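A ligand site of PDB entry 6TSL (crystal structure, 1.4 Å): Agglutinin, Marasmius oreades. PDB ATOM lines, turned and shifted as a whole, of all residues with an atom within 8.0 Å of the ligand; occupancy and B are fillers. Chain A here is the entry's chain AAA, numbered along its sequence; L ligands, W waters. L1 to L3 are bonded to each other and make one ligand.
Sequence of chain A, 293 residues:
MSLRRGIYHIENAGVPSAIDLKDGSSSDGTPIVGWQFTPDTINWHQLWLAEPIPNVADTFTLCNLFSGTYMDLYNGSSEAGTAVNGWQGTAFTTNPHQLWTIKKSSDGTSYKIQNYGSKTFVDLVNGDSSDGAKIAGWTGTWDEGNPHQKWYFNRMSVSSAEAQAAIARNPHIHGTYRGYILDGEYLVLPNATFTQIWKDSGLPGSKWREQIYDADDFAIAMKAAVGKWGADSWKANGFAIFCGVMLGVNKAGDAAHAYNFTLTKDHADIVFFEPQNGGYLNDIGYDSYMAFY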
ATOM      1  N   ALA A  80       7.588 -12.768 -13.219  1.00  0.00           N
ATOM      2  CA  ALA A  80       7.478 -12.168 -11.880  1.00  0.00           C
ATOM      3  C   ALA A  80       6.011 -11.809 -11.604  1.00  0.00           C
ATOM      4  O   ALA A  80       5.350 -11.317 -12.516  1.00  0.00           O
ATOM      5  CB  ALA A  80       8.368 -10.961 -11.772  1.00  0.00           C
ATOM      6  N   GLY A  81       5.491 -12.240 -10.455  1.00  0.00           N
ATOM      7  CA  GLY A  81       4.102 -11.954 -10.050  1.00  0.00           C
ATOM      8  C   GLY A  81       3.174 -13.118 -10.341  1.00  0.00           C
ATOM      9  O   GLY A  81       1.969 -12.973 -10.111  1.00  0.00           O
ATOM     10  N   LYS A 112      15.608 -20.155   0.885  1.00  0.00           N
ATOM     11  CA  LYS A 112      14.844 -19.704  -0.287  1.00  0.00           C
ATOM     12  C   LYS A 112      14.142 -20.902  -0.936  1.00  0.00           C
ATOM     13  O   LYS A 112      14.597 -22.063  -0.717  1.00  0.00           O
ATOM     14  CB  LYS A 112      15.767 -18.997  -1.287  1.00  0.00           C
ATOM     15  CG  LYS A 112      16.536 -17.830  -0.722  1.00  0.00           C
ATOM     16  CD  LYS A 112      17.078 -16.867  -1.786  1.00  0.00           C
ATOM     17  CE  LYS A 112      15.987 -16.242  -2.645  1.00  0.00           C
ATOM     18  NZ  LYS A 112      16.385 -14.919  -3.175  1.00  0.00           N
ATOM     19  N   PHE A 121      11.418 -17.693  -7.520  1.00  0.00           N
ATOM     20  CA  PHE A 121      11.459 -17.888  -6.072  1.00  0.00           C
ATOM     21  C   PHE A 121      10.104 -17.467  -5.459  1.00  0.00           C
ATOM     22  O   PHE A 121       9.528 -16.478  -5.895  1.00  0.00           O
ATOM     23  CB  PHE A 121      12.601 -17.090  -5.469  1.00  0.00           C
ATOM     24  CG  PHE A 121      13.957 -17.662  -5.747  1.00  0.00           C
ATOM     25  CD1 PHE A 121      14.499 -18.634  -4.927  1.00  0.00           C
ATOM     26  CD2 PHE A 121      14.705 -17.236  -6.842  1.00  0.00           C
ATOM     27  CE1 PHE A 121      15.754 -19.183  -5.201  1.00  0.00           C
ATOM     28  CE2 PHE A 121      15.973 -17.748  -7.087  1.00  0.00           C
ATOM     29  CZ  PHE A 121      16.498 -18.704  -6.251  1.00  0.00           C
ATOM     30  N   VAL A 122       9.744 -18.091  -4.362  1.00  0.00           N
ATOM     31  CA  VAL A 122       8.556 -17.702  -3.560  1.00  0.00           C
ATOM     32  C   VAL A 122       8.830 -16.360  -2.893  1.00  0.00           C
ATOM     33  O   VAL A 122       9.781 -16.256  -2.141  1.00  0.00           O
ATOM     34  CB  VAL A 122       8.211 -18.801  -2.525  1.00  0.00           C
ATOM     35  CG1 VAL A 122       7.109 -18.352  -1.574  1.00  0.00           C
ATOM     36  CG2 VAL A 122       7.850 -20.101  -3.216  1.00  0.00           C
ATOM     37  N   ASP A 123       7.956 -15.394  -3.119  1.00  0.00           N
ATOM     38  CA  ASP A 123       8.207 -13.989  -2.801  1.00  0.00           C
ATOM     39  C   ASP A 123       6.965 -13.394  -2.120  1.00  0.00           C
ATOM     40  O   ASP A 123       5.872 -13.441  -2.733  1.00  0.00           O
ATOM     41  CB  ASP A 123       8.606 -13.218  -4.074  1.00  0.00           C
ATOM     42  CG  ASP A 123       9.007 -11.769  -3.834  1.00  0.00           C
ATOM     43  OD1 ASP A 123       8.186 -11.027  -3.247  1.00  0.00           O
ATOM     44  OD2 ASP A 123      10.116 -11.366  -4.312  1.00  0.00           O
ATOM     45  N   LEU A 124       7.106 -12.918  -0.899  1.00  0.00           N
ATOM     46  CA  LEU A 124       6.050 -12.122  -0.233  1.00  0.00           C
ATOM     47  C   LEU A 124       6.049 -10.711  -0.823  1.00  0.00           C
ATOM     48  O   LEU A 124       6.981  -9.964  -0.550  1.00  0.00           O
ATOM     49  CB  LEU A 124       6.313 -12.092   1.264  1.00  0.00           C
ATOM     50  CG  LEU A 124       5.285 -11.341   2.092  1.00  0.00           C
ATOM     51  CD1 LEU A 124       3.913 -11.980   1.995  1.00  0.00           C
ATOM     52  CD2 LEU A 124       5.716 -11.246   3.535  1.00  0.00           C
ATOM     53  N   VAL A 125       5.170 -10.454  -1.771  1.00  0.00           N
ATOM     54  CA  VAL A 125       5.310  -9.297  -2.698  1.00  0.00           C
ATOM     55  C   VAL A 125       5.375  -7.994  -1.859  1.00  0.00           C
ATOM     56  O   VAL A 125       4.473  -7.770  -1.024  1.00  0.00           O
ATOM     57  CB  VAL A 125       4.183  -9.262  -3.728  1.00  0.00           C
ATOM     58  CG1 VAL A 125       4.267  -8.022  -4.609  1.00  0.00           C
ATOM     59  CG2 VAL A 125       4.168 -10.535  -4.567  1.00  0.00           C
ATOM     60  N   ASN A 126       6.459  -7.230  -2.025  1.00  0.00           N
ATOM     61  CA  ASN A 126       6.634  -5.893  -1.399  1.00  0.00           C
ATOM     62  C   ASN A 126       6.890  -6.051   0.099  1.00  0.00           C
ATOM     63  O   ASN A 126       6.852  -5.069   0.771  1.00  0.00           O
ATOM     64  CB  ASN A 126       5.427  -4.983  -1.646  1.00  0.00           C
ATOM     65  CG  ASN A 126       5.436  -4.383  -3.019  1.00  0.00           C
ATOM     66  OD1 ASN A 126       6.501  -4.114  -3.578  1.00  0.00           O
ATOM     67  ND2 ASN A 126       4.259  -4.103  -3.551  1.00  0.00           N
ATOM     68  N   GLY A 127       7.132  -7.261   0.557  1.00  0.00           N
ATOM     69  CA  GLY A 127       7.305  -7.506   2.010  1.00  0.00           C
ATOM     70  C   GLY A 127       6.061  -7.078   2.799  1.00  0.00           C
ATOM     71  O   GLY A 127       6.221  -6.600   3.914  1.00  0.00           O
ATOM     72  N   ASP A 128       4.903  -7.185   2.185  1.00  0.00           N
ATOM     73  CA  ASP A 128       3.635  -6.712   2.781  1.00  0.00           C
ATOM     74  C   ASP A 128       3.277  -7.631   3.966  1.00  0.00           C
ATOM     75  O   ASP A 128       3.081  -8.834   3.738  1.00  0.00           O
ATOM     76  CB  ASP A 128       2.547  -6.693   1.734  1.00  0.00           C
ATOM     77  CG  ASP A 128       1.231  -6.088   2.212  1.00  0.00           C
ATOM     78  OD1 ASP A 128       1.124  -5.811   3.417  1.00  0.00           O
ATOM     79  OD2 ASP A 128       0.328  -5.966   1.394  1.00  0.00           O
ATOM     80  N   LYS A 134      -0.322 -10.995  -1.114  1.00  0.00           N
ATOM     81  CA  LYS A 134       0.018 -11.894  -2.237  1.00  0.00           C
ATOM     82  C   LYS A 134       1.395 -12.543  -1.993  1.00  0.00           C
ATOM     83  O   LYS A 134       2.376 -11.807  -1.706  1.00  0.00           O
ATOM     84  CB  LYS A 134       0.019 -11.114  -3.554  1.00  0.00           C
ATOM     85  CG  LYS A 134       0.354 -11.932  -4.800  1.00  0.00           C
ATOM     86  CD  LYS A 134       0.208 -11.120  -6.095  1.00  0.00           C
ATOM     87  CE  LYS A 134       0.251 -11.977  -7.348  1.00  0.00           C
ATOM     88  NZ  LYS A 134       0.534 -11.146  -8.566  1.00  0.00           N
ATOM     89  N   ALA A 136       3.974 -14.760  -4.561  1.00  0.00           N
ATOM     90  CA  ALA A 136       4.112 -14.966  -6.001  1.00  0.00           C
ATOM     91  C   ALA A 136       5.471 -15.609  -6.307  1.00  0.00           C
ATOM     92  O   ALA A 136       6.383 -15.454  -5.508  1.00  0.00           O
ATOM     93  CB  ALA A 136       3.939 -13.646  -6.728  1.00  0.00           C
ATOM     94  N   GLY A 137       5.579 -16.233  -7.438  1.00  0.00           N
ATOM     95  CA  GLY A 137       6.865 -16.560  -8.030  1.00  0.00           C
ATOM     96  C   GLY A 137       7.530 -15.314  -8.619  1.00  0.00           C
ATOM     97  O   GLY A 137       6.819 -14.487  -9.158  1.00  0.00           O
ATOM     98  N   TRP A 138       8.792 -15.104  -8.305  1.00  0.00           N
ATOM     99  CA  TRP A 138       9.473 -13.839  -8.668  1.00  0.00           C
ATOM    100  C   TRP A 138      10.930 -14.121  -9.054  1.00  0.00           C
ATOM    101  O   TRP A 138      11.530 -15.039  -8.474  1.00  0.00           O
ATOM    102  CB  TRP A 138       9.378 -12.831  -7.519  1.00  0.00           C
ATOM    103  CG  TRP A 138       9.412 -11.411  -7.954  1.00  0.00           C
ATOM    104  CD1 TRP A 138      10.505 -10.673  -8.322  1.00  0.00           C
ATOM    105  CD2 TRP A 138       8.302 -10.506  -7.979  1.00  0.00           C
ATOM    106  NE1 TRP A 138      10.143  -9.411  -8.649  1.00  0.00           N
ATOM    107  CE2 TRP A 138       8.804  -9.258  -8.411  1.00  0.00           C
ATOM    108  CE3 TRP A 138       6.940 -10.630  -7.710  1.00  0.00           C
ATOM    109  CZ2 TRP A 138       7.971  -8.157  -8.597  1.00  0.00           C
ATOM    110  CZ3 TRP A 138       6.133  -9.537  -7.874  1.00  0.00           C
ATOM    111  CH2 TRP A 138       6.648  -8.312  -8.319  1.00  0.00           C
ATOM    112  N   THR A 139      11.459 -13.356  -9.978  1.00  0.00           N
ATOM    113  CA  THR A 139      12.894 -13.361 -10.330  1.00  0.00           C
ATOM    114  C   THR A 139      13.716 -13.246  -9.053  1.00  0.00           C
ATOM    115  O   THR A 139      13.311 -12.467  -8.185  1.00  0.00           O
ATOM    116  CB  THR A 139      13.226 -12.217 -11.285  1.00  0.00           C
ATOM    117  OG1 THR A 139      12.115 -12.067 -12.196  1.00  0.00           O
ATOM    118  CG2 THR A 139      14.504 -12.443 -12.058  1.00  0.00           C
ATOM    119  N   GLY A 140      14.815 -13.938  -8.984  1.00  0.00           N
ATOM    120  CA  GLY A 140      15.781 -13.721  -7.911  1.00  0.00           C
ATOM    121  C   GLY A 140      17.006 -14.573  -8.062  1.00  0.00           C
ATOM    122  O   GLY A 140      17.110 -15.299  -9.074  1.00  0.00           O
ATOM    123  N   THR A 141      17.877 -14.543  -7.063  1.00  0.00           N
ATOM    124  CA  THR A 141      19.126 -15.316  -7.051  1.00  0.00           C
ATOM    125  C   THR A 141      19.238 -16.045  -5.710  1.00  0.00           C
ATOM    126  O   THR A 141      18.662 -15.550  -4.692  1.00  0.00           O
ATOM    127  CB  THR A 141      20.344 -14.408  -7.308  1.00  0.00           C
ATOM    128  OG1 THR A 141      20.551 -13.605  -6.144  1.00  0.00           O
ATOM    129  CG2 THR A 141      20.169 -13.517  -8.524  1.00  0.00           C
ATOM    130  N   GLU A 144      21.349 -13.482  -2.823  1.00  0.00           N
ATOM    131  CA  GLU A 144      21.006 -12.054  -2.489  1.00  0.00           C
ATOM    132  C   GLU A 144      20.322 -11.998  -1.102  1.00  0.00           C
ATOM    133  O   GLU A 144      19.734 -13.017  -0.673  1.00  0.00           O
ATOM    134  CB  GLU A 144      20.132 -11.436  -3.569  1.00  0.00           C
ATOM    135  CG  GLU A 144      18.798 -12.131  -3.731  1.00  0.00           C
ATOM    136  CD  GLU A 144      17.983 -11.622  -4.890  1.00  0.00           C
ATOM    137  OE1 GLU A 144      18.320 -10.503  -5.415  1.00  0.00           O
ATOM    138  OE2 GLU A 144      16.983 -12.278  -5.225  1.00  0.00           O
ATOM    139  N   GLY A 145      20.339 -10.832  -0.470  1.00  0.00           N
ATOM    140  CA  GLY A 145      19.857 -10.648   0.925  1.00  0.00           C
ATOM    141  C   GLY A 145      18.329 -10.432   0.996  1.00  0.00           C
ATOM    142  O   GLY A 145      17.805 -10.446   2.089  1.00  0.00           O
ATOM    143  N   ASN A 146      17.684 -10.163  -0.157  1.00  0.00           N
ATOM    144  CA  ASN A 146      16.262  -9.756  -0.267  1.00  0.00           C
ATOM    145  C   ASN A 146      15.378 -10.555   0.701  1.00  0.00           C
ATOM    146  O   ASN A 146      15.072 -11.693   0.441  1.00  0.00           O
ATOM    147  CB  ASN A 146      15.784  -9.920  -1.708  1.00  0.00           C
ATOM    148  CG  ASN A 146      14.350  -9.500  -1.906  1.00  0.00           C
ATOM    149  OD1 ASN A 146      13.703  -8.973  -0.984  1.00  0.00           O
ATOM    150  ND2 ASN A 146      13.848  -9.663  -3.136  1.00  0.00           N
ATOM    151  N   PRO A 147      14.841  -9.925   1.758  1.00  0.00           N
ATOM    152  CA  PRO A 147      14.034 -10.652   2.754  1.00  0.00           C
ATOM    153  C   PRO A 147      12.628 -11.051   2.239  1.00  0.00           C
ATOM    154  O   PRO A 147      12.025 -11.962   2.822  1.00  0.00           O
ATOM    155  CB  PRO A 147      13.907  -9.671   3.944  1.00  0.00           C
ATOM    156  CG  PRO A 147      14.218  -8.301   3.335  1.00  0.00           C
ATOM    157  CD  PRO A 147      15.153  -8.569   2.176  1.00  0.00           C
ATOM    158  N   HIS A 148      12.161 -10.445   1.141  1.00  0.00           N
ATOM    159  CA  HIS A 148      10.885 -10.856   0.493  1.00  0.00           C
ATOM    160  C   HIS A 148      10.935 -12.350   0.140  1.00  0.00           C
ATOM    161  O   HIS A 148       9.845 -12.973   0.037  1.00  0.00           O
ATOM    162  CB  HIS A 148      10.597  -9.989  -0.736  1.00  0.00           C
ATOM    163  CG  HIS A 148      10.520  -8.531  -0.465  1.00  0.00           C
ATOM    164  ND1 HIS A 148      10.304  -7.605  -1.471  1.00  0.00           N
ATOM    165  CD2 HIS A 148      10.620  -7.826   0.690  1.00  0.00           C
ATOM    166  CE1 HIS A 148      10.265  -6.383  -0.943  1.00  0.00           C
ATOM    167  NE2 HIS A 148      10.467  -6.488   0.368  1.00  0.00           N
ATOM    168  N   GLN A 149      12.118 -12.892  -0.094  1.00  0.00           N
ATOM    169  CA  GLN A 149      12.282 -14.238  -0.666  1.00  0.00           C
ATOM    170  C   GLN A 149      13.021 -15.161   0.348  1.00  0.00           C
ATOM    171  O   GLN A 149      13.390 -16.248  -0.038  1.00  0.00           O
ATOM    172  CB  GLN A 149      13.042 -14.151  -1.996  1.00  0.00           C
ATOM    173  CG  GLN A 149      12.308 -13.339  -3.046  1.00  0.00           C
ATOM    174  CD  GLN A 149      13.002 -13.366  -4.401  1.00  0.00           C
ATOM    175  OE1 GLN A 149      14.078 -13.984  -4.577  1.00  0.00           O
ATOM    176  NE2 GLN A 149      12.378 -12.710  -5.367  1.00  0.00           N
HETATM  177  C1  LIG L   1      14.572  -5.595  -4.199  1.00  0.00           C
HETATM  178  C2  LIG L   1      15.757  -4.852  -4.823  1.00  0.00           C
HETATM  179  C3  LIG L   1      15.365  -3.410  -5.168  1.00  0.00           C
HETATM  180  C4  LIG L   1      14.869  -2.733  -3.938  1.00  0.00           C
HETATM  181  C5  LIG L   1      13.736  -3.546  -3.291  1.00  0.00           C
HETATM  182  C6  LIG L   1      13.265  -2.916  -2.013  1.00  0.00           C
HETATM  183  O1  LIG L   1      16.185  -5.529  -5.990  1.00  0.00           O
HETATM  184  O2  LIG L   1      16.495  -2.686  -5.658  1.00  0.00           O
HETATM  185  O3  LIG L   1      15.950  -2.588  -3.020  1.00  0.00           O
HETATM  186  O4  LIG L   1      14.193  -4.909  -3.025  1.00  0.00           O
HETATM  187  C1  LG2 L   2      11.129  -5.596  -4.576  1.00  0.00           C
HETATM  188  C2  LG2 L   2      12.408  -6.453  -4.725  1.00  0.00           C
HETATM  189  C3  LG2 L   2      12.205  -7.518  -5.770  1.00  0.00           C
HETATM  190  C4  LG2 L   2      10.987  -8.357  -5.378  1.00  0.00           C
HETATM  191  C5  LG2 L   2       9.782  -7.455  -5.254  1.00  0.00           C
HETATM  192  C6  LG2 L   2       8.495  -8.229  -4.862  1.00  0.00           C
HETATM  193  O1  LG2 L   2      10.875  -4.920  -5.782  1.00  0.00           O
HETATM  194  O2  LG2 L   2      13.518  -5.592  -5.093  1.00  0.00           O
HETATM  195  O3  LG2 L   2      13.395  -8.329  -5.861  1.00  0.00           O
HETATM  196  O4  LG2 L   2      11.263  -9.045  -4.135  1.00  0.00           O
HETATM  197  O5  LG2 L   2      10.006  -6.433  -4.269  1.00  0.00           O
HETATM  198  O6  LG2 L   2       8.469  -8.438  -3.463  1.00  0.00           O
HETATM  199  C1  LG3 L   3      13.497  -9.319  -6.732  1.00  0.00           C
HETATM  200  C2  LG3 L   3      14.833  -9.937  -6.825  1.00  0.00           C
HETATM  201  C3  LG3 L   3      15.806  -8.963  -7.514  1.00  0.00           C
HETATM  202  C4  LG3 L   3      15.243  -8.573  -8.846  1.00  0.00           C
HETATM  203  C5  LG3 L   3      13.825  -8.019  -8.657  1.00  0.00           C
HETATM  204  C6  LG3 L   3      13.150  -7.615  -9.961  1.00  0.00           C
HETATM  205  O1  LG3 L   3      15.295 -10.258  -5.495  1.00  0.00           O
HETATM  206  O2  LG3 L   3      17.075  -9.595  -7.655  1.00  0.00           O
HETATM  207  O3  LG3 L   3      15.189  -9.714  -9.718  1.00  0.00           O
HETATM  208  O4  LG3 L   3      13.021  -9.007  -8.005  1.00  0.00           O
HETATM  209  O5  LG3 L   3      11.857  -7.035  -9.696  1.00  0.00           O
HETATM  210  O   HOH W   1       9.680  -7.765 -11.573  1.00  0.00           O
HETATM  211  O   HOH W   2      13.897  -6.248  -0.665  1.00  0.00           O
HETATM  212  O   HOH W   3       9.903  -2.557  -5.064  1.00  0.00           O
HETATM  213  O   HOH W   4      12.741  -4.512  -8.089  1.00  0.00           O
HETATM  214  O   HOH W   5      17.606 -11.431  -9.942  1.00  0.00           O
HETATM  215  O   HOH W   6      17.301  -8.021  -4.461  1.00  0.00           O
HETATM  216  O   HOH W   7      16.513  -9.426 -11.950  1.00  0.00           O
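O6 of LG2 L2 sits at hydrogen-bond distance from ND1 of His 148 (2.8 Å).
The indole nitrogen (NE1) of Trp 138 lies within hydrogen-bond range of an oxygen (O4) of LG3 L3.
An oxygen (O6) of LG2 L2 lies within hydrogen-bond range of the backbone NH (N) of Asn 126, 2.8 Å away.
An oxygen (O1) of LG3 L3 lies within hydrogen-bond range of the side-chain carboxylate (OE2) of Glu 144 (2.6 Å).
The side-chain carboxylate (OD2) of Asp 123 is in hydrogen-bond range of an oxygen (O4) of LG2 L2 (2.6 Å).
An oxygen (O1) of LG3 L3 lies within hydrogen-bond range of the side-chain amide nitrogen of Asn 146, at 2.8 Å.
NZ of Lys 112 is in hydrogen-bond range of OE1 of Gln 149 (2.9 Å).
OE2 of Glu 144 lies close to OE1 of Gln 149 (3.4 Å).
The backbone NH (N) of Thr 141 sits at hydrogen-bond distance from the side-chain carboxylate (OE2) of Glu 144.
The backbone carbonyl oxygen of His 148 sits at hydrogen-bond distance from the backbone NH of Leu 124, 2.9 Å away.
NE2 of His 148 is in hydrogen-bond range of N of Gly 127 (3.4 Å).
The side-chain carboxylate of Glu 144 is in salt-bridge range of the side-chain amino group of Lys 112, 3.4 Å away.
The backbone NH of Asp 123 lies within hydrogen-bond range of the backbone carbonyl oxygen of Ala 136 (2.9 Å).
O of Thr 139 sits at hydrogen-bond distance from NE2 of Gln 149 (3.0 Å).
The backbone carbonyl oxygen (O) of Thr 139 lies close to an oxygen (O4) of LG3 L3 (3.5 Å).
Leu 124 touches the ligand.
Val 125 touches the ligand.
NE2 of Gln 149 touches O1 of LG3 L3 (3.8 Å).
Within 4 Å of the ligand: Asp 123, Leu 124, Val 125, Asn 126, Trp 138, Thr 139, Glu 144, Asn 146, His 148 and Gln 149.
The nearest printed residue that does not touch the ligand is Gly 140 (4.05 Å).
Water W2 bridges O4 of LIG L1 and OD1 of Asn 146.
Water W1 bridges O5 of LG3 L3 (3.0 Å) and NE1 of Trp 138 (3.4 Å).
Water W6 lies within hydrogen-bond range of OE1 of Glu 144 (2.8 Å) and O1 of LIG L1 (3.1 Å).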
